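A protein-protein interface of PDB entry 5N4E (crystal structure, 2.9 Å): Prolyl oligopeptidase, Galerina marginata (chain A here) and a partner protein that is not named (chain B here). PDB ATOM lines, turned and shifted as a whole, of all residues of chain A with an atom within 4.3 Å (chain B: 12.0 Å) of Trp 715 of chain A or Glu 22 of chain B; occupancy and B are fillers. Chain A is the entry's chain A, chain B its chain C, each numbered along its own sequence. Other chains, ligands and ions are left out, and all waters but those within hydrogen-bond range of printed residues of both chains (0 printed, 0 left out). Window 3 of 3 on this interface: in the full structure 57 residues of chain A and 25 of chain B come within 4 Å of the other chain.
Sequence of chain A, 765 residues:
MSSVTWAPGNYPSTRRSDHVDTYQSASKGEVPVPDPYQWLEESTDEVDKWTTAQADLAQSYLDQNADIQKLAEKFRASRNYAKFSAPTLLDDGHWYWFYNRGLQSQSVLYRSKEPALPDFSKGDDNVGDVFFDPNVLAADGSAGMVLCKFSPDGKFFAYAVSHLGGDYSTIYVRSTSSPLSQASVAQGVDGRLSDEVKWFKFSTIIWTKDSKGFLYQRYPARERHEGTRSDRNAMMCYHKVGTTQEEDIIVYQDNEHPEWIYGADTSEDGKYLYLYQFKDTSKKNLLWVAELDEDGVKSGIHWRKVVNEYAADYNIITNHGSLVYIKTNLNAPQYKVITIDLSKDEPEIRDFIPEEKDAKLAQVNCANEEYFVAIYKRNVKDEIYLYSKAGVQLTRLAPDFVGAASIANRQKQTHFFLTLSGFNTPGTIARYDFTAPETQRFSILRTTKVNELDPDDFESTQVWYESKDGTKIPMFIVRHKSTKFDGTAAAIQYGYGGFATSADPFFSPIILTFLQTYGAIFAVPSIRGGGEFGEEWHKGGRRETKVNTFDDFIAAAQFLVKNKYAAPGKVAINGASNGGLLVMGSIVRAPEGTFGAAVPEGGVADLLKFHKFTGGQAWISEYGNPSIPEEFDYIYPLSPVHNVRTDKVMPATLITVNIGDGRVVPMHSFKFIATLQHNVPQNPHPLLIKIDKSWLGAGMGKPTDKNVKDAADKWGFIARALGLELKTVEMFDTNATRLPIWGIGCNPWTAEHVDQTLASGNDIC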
ATOM      1  N   LEU A  71     -11.546 -34.582 -27.230  1.00  0.00           N
ATOM      2  CA  LEU A  71     -11.231 -33.220 -26.775  1.00  0.00           C
ATOM      3  C   LEU A  71     -10.613 -32.354 -27.877  1.00  0.00           C
ATOM      4  O   LEU A  71     -10.913 -31.162 -27.958  1.00  0.00           O
ATOM      5  CB  LEU A  71     -10.299 -33.233 -25.554  1.00  0.00           C
ATOM      6  CG  LEU A  71     -10.865 -33.680 -24.205  1.00  0.00           C
ATOM      7  CD1 LEU A  71      -9.760 -33.608 -23.165  1.00  0.00           C
ATOM      8  CD2 LEU A  71     -12.056 -32.836 -23.774  1.00  0.00           C
ATOM      9  N   PHE A  75     -11.896 -28.779 -28.820  1.00  0.00           N
ATOM     10  CA  PHE A  75     -10.987 -27.630 -28.712  1.00  0.00           C
ATOM     11  C   PHE A  75     -10.751 -26.919 -30.042  1.00  0.00           C
ATOM     12  O   PHE A  75     -10.635 -25.694 -30.065  1.00  0.00           O
ATOM     13  CB  PHE A  75      -9.630 -28.034 -28.105  1.00  0.00           C
ATOM     14  CG  PHE A  75      -9.687 -28.513 -26.664  1.00  0.00           C
ATOM     15  CD1 PHE A  75      -8.610 -29.227 -26.130  1.00  0.00           C
ATOM     16  CD2 PHE A  75     -10.784 -28.261 -25.834  1.00  0.00           C
ATOM     17  CE1 PHE A  75      -8.628 -29.674 -24.811  1.00  0.00           C
ATOM     18  CE2 PHE A  75     -10.802 -28.709 -24.521  1.00  0.00           C
ATOM     19  CZ  PHE A  75      -9.726 -29.413 -24.008  1.00  0.00           C
ATOM     20  N   ILE A 492      -9.122 -26.898 -11.741  1.00  0.00           N
ATOM     21  CA  ILE A 492      -7.867 -26.657 -12.441  1.00  0.00           C
ATOM     22  C   ILE A 492      -7.315 -25.328 -11.944  1.00  0.00           C
ATOM     23  O   ILE A 492      -7.908 -24.275 -12.179  1.00  0.00           O
ATOM     24  CB  ILE A 492      -8.047 -26.599 -13.967  1.00  0.00           C
ATOM     25  CG1 ILE A 492      -8.950 -27.754 -14.449  1.00  0.00           C
ATOM     26  CG2 ILE A 492      -6.672 -26.582 -14.633  1.00  0.00           C
ATOM     27  CD1 ILE A 492      -8.313 -29.131 -14.419  1.00  0.00           C
ATOM     28  N   TYR A 494      -4.509 -22.532 -11.905  1.00  0.00           N
ATOM     29  CA  TYR A 494      -3.428 -21.885 -12.657  1.00  0.00           C
ATOM     30  C   TYR A 494      -2.663 -20.903 -11.794  1.00  0.00           C
ATOM     31  O   TYR A 494      -3.231 -20.276 -10.902  1.00  0.00           O
ATOM     32  CB  TYR A 494      -3.984 -21.127 -13.861  1.00  0.00           C
ATOM     33  CG  TYR A 494      -4.023 -21.909 -15.149  1.00  0.00           C
ATOM     34  CD1 TYR A 494      -3.705 -21.294 -16.353  1.00  0.00           C
ATOM     35  CD2 TYR A 494      -4.391 -23.258 -15.177  1.00  0.00           C
ATOM     36  CE1 TYR A 494      -3.750 -21.987 -17.552  1.00  0.00           C
ATOM     37  CE2 TYR A 494      -4.447 -23.959 -16.374  1.00  0.00           C
ATOM     38  CZ  TYR A 494      -4.127 -23.318 -17.557  1.00  0.00           C
ATOM     39  OH  TYR A 494      -4.160 -24.014 -18.741  1.00  0.00           O
ATOM     40  N   PHE A 506      -8.363 -13.552 -18.510  1.00  0.00           N
ATOM     41  CA  PHE A 506      -8.105 -13.769 -19.932  1.00  0.00           C
ATOM     42  C   PHE A 506      -9.142 -14.747 -20.478  1.00  0.00           C
ATOM     43  O   PHE A 506      -9.601 -15.633 -19.745  1.00  0.00           O
ATOM     44  CB  PHE A 506      -6.687 -14.314 -20.146  1.00  0.00           C
ATOM     45  CG  PHE A 506      -6.475 -15.708 -19.609  1.00  0.00           C
ATOM     46  CD1 PHE A 506      -6.329 -15.929 -18.241  1.00  0.00           C
ATOM     47  CD2 PHE A 506      -6.422 -16.805 -20.469  1.00  0.00           C
ATOM     48  CE1 PHE A 506      -6.135 -17.209 -17.742  1.00  0.00           C
ATOM     49  CE2 PHE A 506      -6.233 -18.090 -19.974  1.00  0.00           C
ATOM     50  CZ  PHE A 506      -6.088 -18.293 -18.609  1.00  0.00           C
ATOM     51  N   SER A 508     -10.139 -17.880 -22.630  1.00  0.00           N
ATOM     52  CA  SER A 508      -9.636 -19.117 -23.208  1.00  0.00           C
ATOM     53  C   SER A 508     -10.831 -19.986 -23.601  1.00  0.00           C
ATOM     54  O   SER A 508     -11.502 -20.523 -22.721  1.00  0.00           O
ATOM     55  CB  SER A 508      -8.763 -19.846 -22.190  1.00  0.00           C
ATOM     56  OG  SER A 508      -8.410 -21.146 -22.639  1.00  0.00           O
ATOM     57  N   ILE A 510     -10.681 -22.889 -24.933  1.00  0.00           N
ATOM     58  CA  ILE A 510     -10.307 -24.262 -24.574  1.00  0.00           C
ATOM     59  C   ILE A 510     -10.617 -24.567 -23.104  1.00  0.00           C
ATOM     60  O   ILE A 510     -11.144 -25.640 -22.798  1.00  0.00           O
ATOM     61  CB  ILE A 510      -8.825 -24.558 -24.939  1.00  0.00           C
ATOM     62  CG1 ILE A 510      -8.706 -24.657 -26.468  1.00  0.00           C
ATOM     63  CG2 ILE A 510      -8.322 -25.841 -24.275  1.00  0.00           C
ATOM     64  CD1 ILE A 510      -7.303 -24.821 -27.003  1.00  0.00           C
ATOM     65  N   ILE A 511     -10.292 -23.632 -22.210  1.00  0.00           N
ATOM     66  CA  ILE A 511     -10.583 -23.783 -20.775  1.00  0.00           C
ATOM     67  C   ILE A 511     -12.090 -23.869 -20.548  1.00  0.00           C
ATOM     68  O   ILE A 511     -12.563 -24.821 -19.932  1.00  0.00           O
ATOM     69  CB  ILE A 511      -9.950 -22.649 -19.925  1.00  0.00           C
ATOM     70  CG1 ILE A 511      -8.434 -22.851 -19.856  1.00  0.00           C
ATOM     71  CG2 ILE A 511     -10.540 -22.605 -18.511  1.00  0.00           C
ATOM     72  CD1 ILE A 511      -7.648 -21.683 -19.294  1.00  0.00           C
ATOM     73  N   PHE A 514     -13.420 -27.111 -21.631  1.00  0.00           N
ATOM     74  CA  PHE A 514     -13.087 -28.140 -20.639  1.00  0.00           C
ATOM     75  C   PHE A 514     -14.007 -28.075 -19.419  1.00  0.00           C
ATOM     76  O   PHE A 514     -14.420 -29.118 -18.908  1.00  0.00           O
ATOM     77  CB  PHE A 514     -11.615 -28.045 -20.218  1.00  0.00           C
ATOM     78  CG  PHE A 514     -11.178 -29.136 -19.278  1.00  0.00           C
ATOM     79  CD1 PHE A 514     -10.698 -30.351 -19.761  1.00  0.00           C
ATOM     80  CD2 PHE A 514     -11.236 -28.944 -17.904  1.00  0.00           C
ATOM     81  CE1 PHE A 514     -10.292 -31.349 -18.890  1.00  0.00           C
ATOM     82  CE2 PHE A 514     -10.831 -29.939 -17.026  1.00  0.00           C
ATOM     83  CZ  PHE A 514     -10.362 -31.146 -17.520  1.00  0.00           C
ATOM     84  N   ALA A 711      -2.942 -29.209 -26.482  1.00  0.00           N
ATOM     85  CA  ALA A 711      -4.007 -28.905 -25.524  1.00  0.00           C
ATOM     86  C   ALA A 711      -4.822 -30.159 -25.207  1.00  0.00           C
ATOM     87  O   ALA A 711      -5.031 -30.492 -24.044  1.00  0.00           O
ATOM     88  CB  ALA A 711      -4.907 -27.802 -26.057  1.00  0.00           C
ATOM     89  N   ALA A 712      -5.244 -30.869 -26.252  1.00  0.00           N
ATOM     90  CA  ALA A 712      -5.987 -32.122 -26.091  1.00  0.00           C
ATOM     91  C   ALA A 712      -5.241 -33.168 -25.250  1.00  0.00           C
ATOM     92  O   ALA A 712      -5.869 -33.884 -24.465  1.00  0.00           O
ATOM     93  CB  ALA A 712      -6.347 -32.697 -27.450  1.00  0.00           C
ATOM     94  N   ASP A 713      -3.917 -33.243 -25.415  1.00  0.00           N
ATOM     95  CA  ASP A 713      -3.066 -34.135 -24.609  1.00  0.00           C
ATOM     96  C   ASP A 713      -3.038 -33.730 -23.130  1.00  0.00           C
ATOM     97  O   ASP A 713      -3.271 -34.560 -22.245  1.00  0.00           O
ATOM     98  CB  ASP A 713      -1.614 -34.158 -25.148  1.00  0.00           C
ATOM     99  CG  ASP A 713      -1.430 -35.073 -26.367  1.00  0.00           C
ATOM    100  OD1 ASP A 713      -0.406 -34.915 -27.075  1.00  0.00           O
ATOM    101  OD2 ASP A 713      -2.268 -35.962 -26.608  1.00  0.00           O
ATOM    102  N   LYS A 714      -2.743 -32.454 -22.883  1.00  0.00           N
ATOM    103  CA  LYS A 714      -2.644 -31.910 -21.522  1.00  0.00           C
ATOM    104  C   LYS A 714      -3.941 -32.070 -20.730  1.00  0.00           C
ATOM    105  O   LYS A 714      -3.941 -32.620 -19.629  1.00  0.00           O
ATOM    106  CB  LYS A 714      -2.251 -30.422 -21.564  1.00  0.00           C
ATOM    107  CG  LYS A 714      -2.400 -29.695 -20.235  1.00  0.00           C
ATOM    108  CD  LYS A 714      -1.675 -28.359 -20.209  1.00  0.00           C
ATOM    109  CE  LYS A 714      -2.365 -27.295 -21.051  1.00  0.00           C
ATOM    110  NZ  LYS A 714      -2.246 -25.934 -20.444  1.00  0.00           N
ATOM    111  N   TRP A 715      -5.030 -31.562 -21.297  1.00  0.00           N
ATOM    112  CA  TRP A 715      -6.336 -31.559 -20.631  1.00  0.00           C
ATOM    113  C   TRP A 715      -6.959 -32.957 -20.541  1.00  0.00           C
ATOM    114  O   TRP A 715      -7.681 -33.247 -19.588  1.00  0.00           O
ATOM    115  CB  TRP A 715      -7.287 -30.578 -21.325  1.00  0.00           C
ATOM    116  CG  TRP A 715      -6.876 -29.134 -21.167  1.00  0.00           C
ATOM    117  CD1 TRP A 715      -6.195 -28.368 -22.067  1.00  0.00           C
ATOM    118  CD2 TRP A 715      -7.111 -28.297 -20.033  1.00  0.00           C
ATOM    119  NE1 TRP A 715      -5.998 -27.105 -21.569  1.00  0.00           N
ATOM    120  CE2 TRP A 715      -6.549 -27.033 -20.321  1.00  0.00           C
ATOM    121  CE3 TRP A 715      -7.748 -28.489 -18.802  1.00  0.00           C
ATOM    122  CZ2 TRP A 715      -6.607 -25.967 -19.426  1.00  0.00           C
ATOM    123  CZ3 TRP A 715      -7.805 -27.429 -17.917  1.00  0.00           C
ATOM    124  CH2 TRP A 715      -7.239 -26.182 -18.230  1.00  0.00           C
ATOM    125  N   GLY A 716      -6.680 -33.815 -21.521  1.00  0.00           N
ATOM    126  CA  GLY A 716      -7.072 -35.224 -21.457  1.00  0.00           C
ATOM    127  C   GLY A 716      -6.340 -36.006 -20.379  1.00  0.00           C
ATOM    128  O   GLY A 716      -6.942 -36.839 -19.692  1.00  0.00           O
ATOM    129  N   PHE A 717      -5.038 -35.741 -20.236  1.00  0.00           N
ATOM    130  CA  PHE A 717      -4.228 -36.328 -19.160  1.00  0.00           C
ATOM    131  C   PHE A 717      -4.759 -35.950 -17.776  1.00  0.00           C
ATOM    132  O   PHE A 717      -4.828 -36.798 -16.885  1.00  0.00           O
ATOM    133  CB  PHE A 717      -2.757 -35.905 -19.286  1.00  0.00           C
ATOM    134  CG  PHE A 717      -1.863 -36.482 -18.219  1.00  0.00           C
ATOM    135  CD1 PHE A 717      -1.290 -37.742 -18.374  1.00  0.00           C
ATOM    136  CD2 PHE A 717      -1.605 -35.770 -17.049  1.00  0.00           C
ATOM    137  CE1 PHE A 717      -0.482 -38.277 -17.383  1.00  0.00           C
ATOM    138  CE2 PHE A 717      -0.794 -36.300 -16.058  1.00  0.00           C
ATOM    139  CZ  PHE A 717      -0.231 -37.553 -16.228  1.00  0.00           C
ATOM    140  N   ILE A 718      -5.108 -34.676 -17.605  1.00  0.00           N
ATOM    141  CA  ILE A 718      -5.683 -34.190 -16.350  1.00  0.00           C
ATOM    142  C   ILE A 718      -7.038 -34.854 -16.118  1.00  0.00           C
ATOM    143  O   ILE A 718      -7.295 -35.358 -15.028  1.00  0.00           O
ATOM    144  CB  ILE A 718      -5.814 -32.645 -16.328  1.00  0.00           C
ATOM    145  CG1 ILE A 718      -4.416 -32.001 -16.295  1.00  0.00           C
ATOM    146  CG2 ILE A 718      -6.643 -32.172 -15.126  1.00  0.00           C
ATOM    147  CD1 ILE A 718      -4.389 -30.549 -16.722  1.00  0.00           C
ATOM    148  N   ALA A 719      -7.884 -34.864 -17.148  1.00  0.00           N
ATOM    149  CA  ALA A 719      -9.217 -35.472 -17.064  1.00  0.00           C
ATOM    150  C   ALA A 719      -9.156 -36.922 -16.579  1.00  0.00           C
ATOM    151  O   ALA A 719      -9.869 -37.295 -15.641  1.00  0.00           O
ATOM    152  CB  ALA A 719      -9.927 -35.394 -18.406  1.00  0.00           C
ATOM    153  N   ILE B  11       8.573 -16.713 -18.864  1.00  0.00           N
ATOM    154  CA  ILE B  11       7.128 -16.624 -19.119  1.00  0.00           C
ATOM    155  C   ILE B  11       6.825 -17.256 -20.483  1.00  0.00           C
ATOM    156  O   ILE B  11       7.703 -17.297 -21.351  1.00  0.00           O
ATOM    157  CB  ILE B  11       6.639 -15.151 -19.056  1.00  0.00           C
ATOM    158  CG1 ILE B  11       5.109 -15.079 -18.954  1.00  0.00           C
ATOM    159  CG2 ILE B  11       7.154 -14.337 -20.244  1.00  0.00           C
ATOM    160  CD1 ILE B  11       4.586 -13.719 -18.549  1.00  0.00           C
ATOM    161  N   TRP B  12       5.596 -17.745 -20.668  1.00  0.00           N
ATOM    162  CA  TRP B  12       5.236 -18.534 -21.856  1.00  0.00           C
ATOM    163  C   TRP B  12       5.398 -17.815 -23.207  1.00  0.00           C
ATOM    164  O   TRP B  12       6.040 -18.367 -24.114  1.00  0.00           O
ATOM    165  CB  TRP B  12       3.811 -19.084 -21.746  1.00  0.00           C
ATOM    166  CG  TRP B  12       3.476 -20.049 -22.850  1.00  0.00           C
ATOM    167  CD1 TRP B  12       3.851 -21.357 -22.928  1.00  0.00           C
ATOM    168  CD2 TRP B  12       2.723 -19.775 -24.041  1.00  0.00           C
ATOM    169  NE1 TRP B  12       3.369 -21.923 -24.083  1.00  0.00           N
ATOM    170  CE2 TRP B  12       2.678 -20.975 -24.789  1.00  0.00           C
ATOM    171  CE3 TRP B  12       2.078 -18.635 -24.549  1.00  0.00           C
ATOM    172  CZ2 TRP B  12       2.008 -21.073 -26.016  1.00  0.00           C
ATOM    173  CZ3 TRP B  12       1.415 -18.733 -25.778  1.00  0.00           C
ATOM    174  CH2 TRP B  12       1.385 -19.947 -26.492  1.00  0.00           C
ATOM    175  N   GLY B  13       4.823 -16.623 -23.341  1.00  0.00           N
ATOM    176  CA  GLY B  13       4.802 -15.930 -24.635  1.00  0.00           C
ATOM    177  C   GLY B  13       4.404 -14.477 -24.556  1.00  0.00           C
ATOM    178  O   GLY B  13       3.611 -14.087 -23.694  1.00  0.00           O
ATOM    179  N   ILE B  14       4.944 -13.681 -25.486  1.00  0.00           N
ATOM    180  CA  ILE B  14       4.696 -12.223 -25.564  1.00  0.00           C
ATOM    181  C   ILE B  14       3.548 -11.915 -26.534  1.00  0.00           C
ATOM    182  O   ILE B  14       3.752 -11.632 -27.715  1.00  0.00           O
ATOM    183  CB  ILE B  14       5.999 -11.415 -25.899  1.00  0.00           C
ATOM    184  CG1 ILE B  14       5.741  -9.901 -26.082  1.00  0.00           C
ATOM    185  CG2 ILE B  14       6.753 -11.981 -27.108  1.00  0.00           C
ATOM    186  CD1 ILE B  14       5.017  -9.219 -24.938  1.00  0.00           C
ATOM    187  N   TRP B  19       0.842 -15.199 -19.756  1.00  0.00           N
ATOM    188  CA  TRP B  19       1.383 -15.924 -18.598  1.00  0.00           C
ATOM    189  C   TRP B  19       1.011 -17.420 -18.529  1.00  0.00           C
ATOM    190  O   TRP B  19       1.338 -18.084 -17.543  1.00  0.00           O
ATOM    191  CB  TRP B  19       1.018 -15.203 -17.280  1.00  0.00           C
ATOM    192  CG  TRP B  19      -0.457 -15.111 -16.965  1.00  0.00           C
ATOM    193  CD1 TRP B  19      -1.330 -14.152 -17.395  1.00  0.00           C
ATOM    194  CD2 TRP B  19      -1.217 -15.992 -16.123  1.00  0.00           C
ATOM    195  NE1 TRP B  19      -2.587 -14.391 -16.894  1.00  0.00           N
ATOM    196  CE2 TRP B  19      -2.548 -15.514 -16.111  1.00  0.00           C
ATOM    197  CE3 TRP B  19      -0.905 -17.146 -15.388  1.00  0.00           C
ATOM    198  CZ2 TRP B  19      -3.570 -16.150 -15.388  1.00  0.00           C
ATOM    199  CZ3 TRP B  19      -1.927 -17.784 -14.671  1.00  0.00           C
ATOM    200  CH2 TRP B  19      -3.241 -17.279 -14.678  1.00  0.00           C
ATOM    201  N   THR B  20       0.346 -17.945 -19.566  1.00  0.00           N
ATOM    202  CA  THR B  20      -0.056 -19.364 -19.632  1.00  0.00           C
ATOM    203  C   THR B  20       0.065 -19.908 -21.055  1.00  0.00           C
ATOM    204  O   THR B  20       0.268 -19.151 -22.006  1.00  0.00           O
ATOM    205  CB  THR B  20      -1.526 -19.610 -19.192  1.00  0.00           C
ATOM    206  OG1 THR B  20      -2.429 -19.223 -20.232  1.00  0.00           O
ATOM    207  CG2 THR B  20      -1.886 -18.864 -17.935  1.00  0.00           C
ATOM    208  N   ALA B  21      -0.092 -21.223 -21.186  1.00  0.00           N
ATOM    209  CA  ALA B  21      -0.156 -21.880 -22.496  1.00  0.00           C
ATOM    210  C   ALA B  21      -1.451 -21.564 -23.265  1.00  0.00           C
ATOM    211  O   ALA B  21      -1.459 -21.625 -24.489  1.00  0.00           O
ATOM    212  CB  ALA B  21       0.017 -23.384 -22.345  1.00  0.00           C
ATOM    213  N   GLU B  22      -2.526 -21.228 -22.547  1.00  0.00           N
ATOM    214  CA  GLU B  22      -3.825 -20.897 -23.162  1.00  0.00           C
ATOM    215  C   GLU B  22      -3.937 -19.445 -23.664  1.00  0.00           C
ATOM    216  O   GLU B  22      -4.941 -19.085 -24.282  1.00  0.00           O
ATOM    217  CB  GLU B  22      -4.980 -21.224 -22.202  1.00  0.00           C
ATOM    218  CG  GLU B  22      -5.512 -22.660 -22.307  1.00  0.00           C
ATOM    219  CD  GLU B  22      -4.471 -23.723 -22.030  1.00  0.00           C
ATOM    220  OE1 GLU B  22      -4.584 -24.823 -22.607  1.00  0.00           O
ATOM    221  OE2 GLU B  22      -3.538 -23.466 -21.240  1.00  0.00           O
ATOM    222  N   HIS B  23      -2.912 -18.629 -23.419  1.00  0.00           N
ATOM    223  CA  HIS B  23      -2.798 -17.304 -24.051  1.00  0.00           C
ATOM    224  C   HIS B  23      -2.448 -17.364 -25.559  1.00  0.00           C
ATOM    225  O   HIS B  23      -2.254 -16.315 -26.185  1.00  0.00           O
ATOM    226  CB  HIS B  23      -1.763 -16.438 -23.298  1.00  0.00           C
ATOM    227  CG  HIS B  23      -2.256 -15.901 -21.989  1.00  0.00           C
ATOM    228  ND1 HIS B  23      -2.334 -16.668 -20.848  1.00  0.00           N
ATOM    229  CD2 HIS B  23      -2.691 -14.666 -21.641  1.00  0.00           C
ATOM    230  CE1 HIS B  23      -2.807 -15.937 -19.857  1.00  0.00           C
ATOM    231  NE2 HIS B  23      -3.028 -14.716 -20.310  1.00  0.00           N
ATOM    232  N   VAL B  24      -2.345 -18.575 -26.127  1.00  0.00           N
ATOM    233  CA  VAL B  24      -2.013 -18.840 -27.547  1.00  0.00           C
ATOM    234  C   VAL B  24      -2.360 -17.705 -28.527  1.00  0.00           C
ATOM    235  O   VAL B  24      -1.512 -17.341 -29.345  1.00  0.00           O
ATOM    236  CB  VAL B  24      -2.678 -20.160 -28.100  1.00  0.00           C
ATOM    237  CG1 VAL B  24      -2.076 -20.562 -29.452  1.00  0.00           C
ATOM    238  CG2 VAL B  24      -2.553 -21.342 -27.152  1.00  0.00           C
ATOM    239  N   ASP B  25      -3.582 -17.164 -28.459  1.00  0.00           N
ATOM    240  CA  ASP B  25      -4.000 -16.119 -29.385  1.00  0.00           C
ATOM    241  C   ASP B  25      -3.922 -14.720 -28.772  1.00  0.00           C
ATOM    242  O   ASP B  25      -4.701 -14.365 -27.887  1.00  0.00           O
ATOM    243  CB  ASP B  25      -5.404 -16.382 -29.930  1.00  0.00           C
ATOM    244  CG  ASP B  25      -5.627 -15.714 -31.275  1.00  0.00           C
ATOM    245  OD1 ASP B  25      -6.090 -14.555 -31.289  1.00  0.00           O
ATOM    246  OD2 ASP B  25      -5.281 -16.324 -32.310  1.00  0.00           O
ATOM    247  N   GLN B  26      -2.964 -13.936 -29.267  1.00  0.00           N
ATOM    248  CA  GLN B  26      -2.756 -12.550 -28.870  1.00  0.00           C
ATOM    249  C   GLN B  26      -3.196 -11.566 -29.966  1.00  0.00           C
ATOM    250  O   GLN B  26      -2.681 -10.452 -30.034  1.00  0.00           O
ATOM    251  CB  GLN B  26      -1.266 -12.336 -28.545  1.00  0.00           C
ATOM    252  CG  GLN B  26      -0.690 -13.206 -27.431  1.00  0.00           C
ATOM    253  CD  GLN B  26      -1.149 -12.783 -26.052  1.00  0.00           C
ATOM    254  OE1 GLN B  26      -1.664 -13.583 -25.277  1.00  0.00           O
ATOM    255  NE2 GLN B  26      -0.941 -11.508 -25.728  1.00  0.00           N
ATOM    256  N   THR B  27      -4.158 -11.964 -30.805  1.00  0.00           N
ATOM    257  CA  THR B  27      -4.618 -11.132 -31.916  1.00  0.00           C
ATOM    258  C   THR B  27      -5.340  -9.869 -31.430  1.00  0.00           C
ATOM    259  O   THR B  27      -5.189  -8.810 -32.037  1.00  0.00           O
ATOM    260  CB  THR B  27      -5.546 -11.912 -32.879  1.00  0.00           C
ATOM    261  OG1 THR B  27      -4.926 -13.148 -33.258  1.00  0.00           O
ATOM    262  CG2 THR B  27      -5.854 -11.093 -34.143  1.00  0.00           C
ATOM    263  N   LEU B  28      -6.101  -9.981 -30.340  1.00  0.00           N
ATOM    264  CA  LEU B  28      -6.870  -8.855 -29.791  1.00  0.00           C
ATOM    265  C   LEU B  28      -6.019  -7.621 -29.481  1.00  0.00           C
ATOM    266  O   LEU B  28      -6.400  -6.499 -29.834  1.00  0.00           O
ATOM    267  CB  LEU B  28      -7.620  -9.282 -28.524  1.00  0.00           C
ATOM    268  CG  LEU B  28      -8.552  -8.256 -27.873  1.00  0.00           C
ATOM    269  CD1 LEU B  28      -9.690  -7.875 -28.812  1.00  0.00           C
ATOM    270  CD2 LEU B  28      -9.083  -8.804 -26.559  1.00  0.00           C
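The side-chain carboxylate of Glu 22 of chain B lies within hydrogen-bond range of the side-chain hydroxyl of Tyr 494 of chain A, at 2.6 Å.
NZ of Lys 714 of chain A is in salt-bridge range of OE2 of Glu 22 of chain B.
The indole nitrogen of Trp 715 of chain A sits at hydrogen-bond distance from the side-chain carboxylate of Glu 22 of chain B (2.9 Å).
The indole nitrogen (NE1) of Trp 19 of chain B lies close to a ring nitrogen (NE2) of His 23 of chain B (3.5 Å).
The side-chain hydroxyl (OH) of Tyr 494 of chain A sits at hydrogen-bond distance from the side-chain amino group (NZ) of Lys 714 of chain A (3.2 Å).
ND1 of His 23 of chain B sits at hydrogen-bond distance from OG1 of Thr 20 of chain B, at 2.6 Å.
N of Ile 511 of chain A is in hydrogen-bond range of OG of Ser 508 of chain A (3.1 Å).
The backbone NH (N) of Glu 22 of chain B lies within hydrogen-bond range of the side-chain hydroxyl (OG1) of Thr 20 of chain B, 3.1 Å away.
The backbone carbonyl oxygen of His 23 of chain B lies close to the side-chain amide oxygen of Gln 26 of chain B.
Thr 20 of chain B touches Tyr 494 of chain A (CG2 to CD1, 3.4 Å).
Phe 506 of chain A touches Trp 19 of chain B.
Thr 20 of chain B touches Phe 506 of chain A.
NE2 of His 23 of chain B touches CG of Phe 506 of chain A, at 3.7 Å.
OG of Ser 508 of chain A touches CG of Glu 22 of chain B, 3.3 Å away.
Glu 22 of chain B touches Ile 511 of chain A (CG to CG1, 3.8 Å).
CB of Ala 21 of chain B touches NZ of Lys 714 of chain A, at 3.9 Å.
No residue of chain B comes within 4 Å of Ile 492 of chain A.
Printed residues of chain B within 4 Å of Tyr 494 of chain A: Thr 20 (3.4 Å) and Glu 22 (2.6 Å).
Of the printed residues of chain B, Phe 506 of chain A touches Trp 19, Thr 20 and His 23.
No residue of chain B comes within 4 Å of Ile 510 of chain A.
Ile 511 of chain A touches just one residue of chain B: Glu 22 (3.8 Å).
Phe 514 of chain A touches none of the printed residues of chain B.
No residue of chain B comes within 4 Å of Ala 711 of chain A.
No residue of chain B comes within 4 Å of Ala 712 of chain A.
Of chain B, only Glu 22 (2.9 Å) comes within 4 Å of Trp 715 of chain A.
Gly 716 of chain A touches none of the printed residues of chain B.
No residue of chain B comes within 4 Å of Ile 718 of chain A.
No residue of chain B comes within 4 Å of Ala 719 of chain A.
Of the printed residues of chain A, Ala 21 of chain B touches Lys 714.
Glu 22 of chain B touches just these residues of chain A: Tyr 494 (2.6 Å), Ser 508 (3.3 Å), Ile 511 (3.8 Å), Lys 714 (2.9 Å) and Trp 715 (2.9 Å).
The nearest residue of chain A that does not touch Glu 22 of chain B is Phe 506 of chain A (4.04 Å).
The nearest printed residue of chain A that does not touch Ala 21 of chain B is Tyr 494 of chain A (5.2 Å).
Hydrophobic or aromatic side chains of chain B within 4 Å of the printed part of chain A: Trp 19, Ala 21 and His 23.
Among the printed residues, 10 pairs touch across the chains.
Among the printed residues, Asp or Glu carboxylates within 4 Å of a Lys or Arg side-chain nitrogen of the other chain: Lys 714 of chain A with Glu 22 of chain B (2.9 Å).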
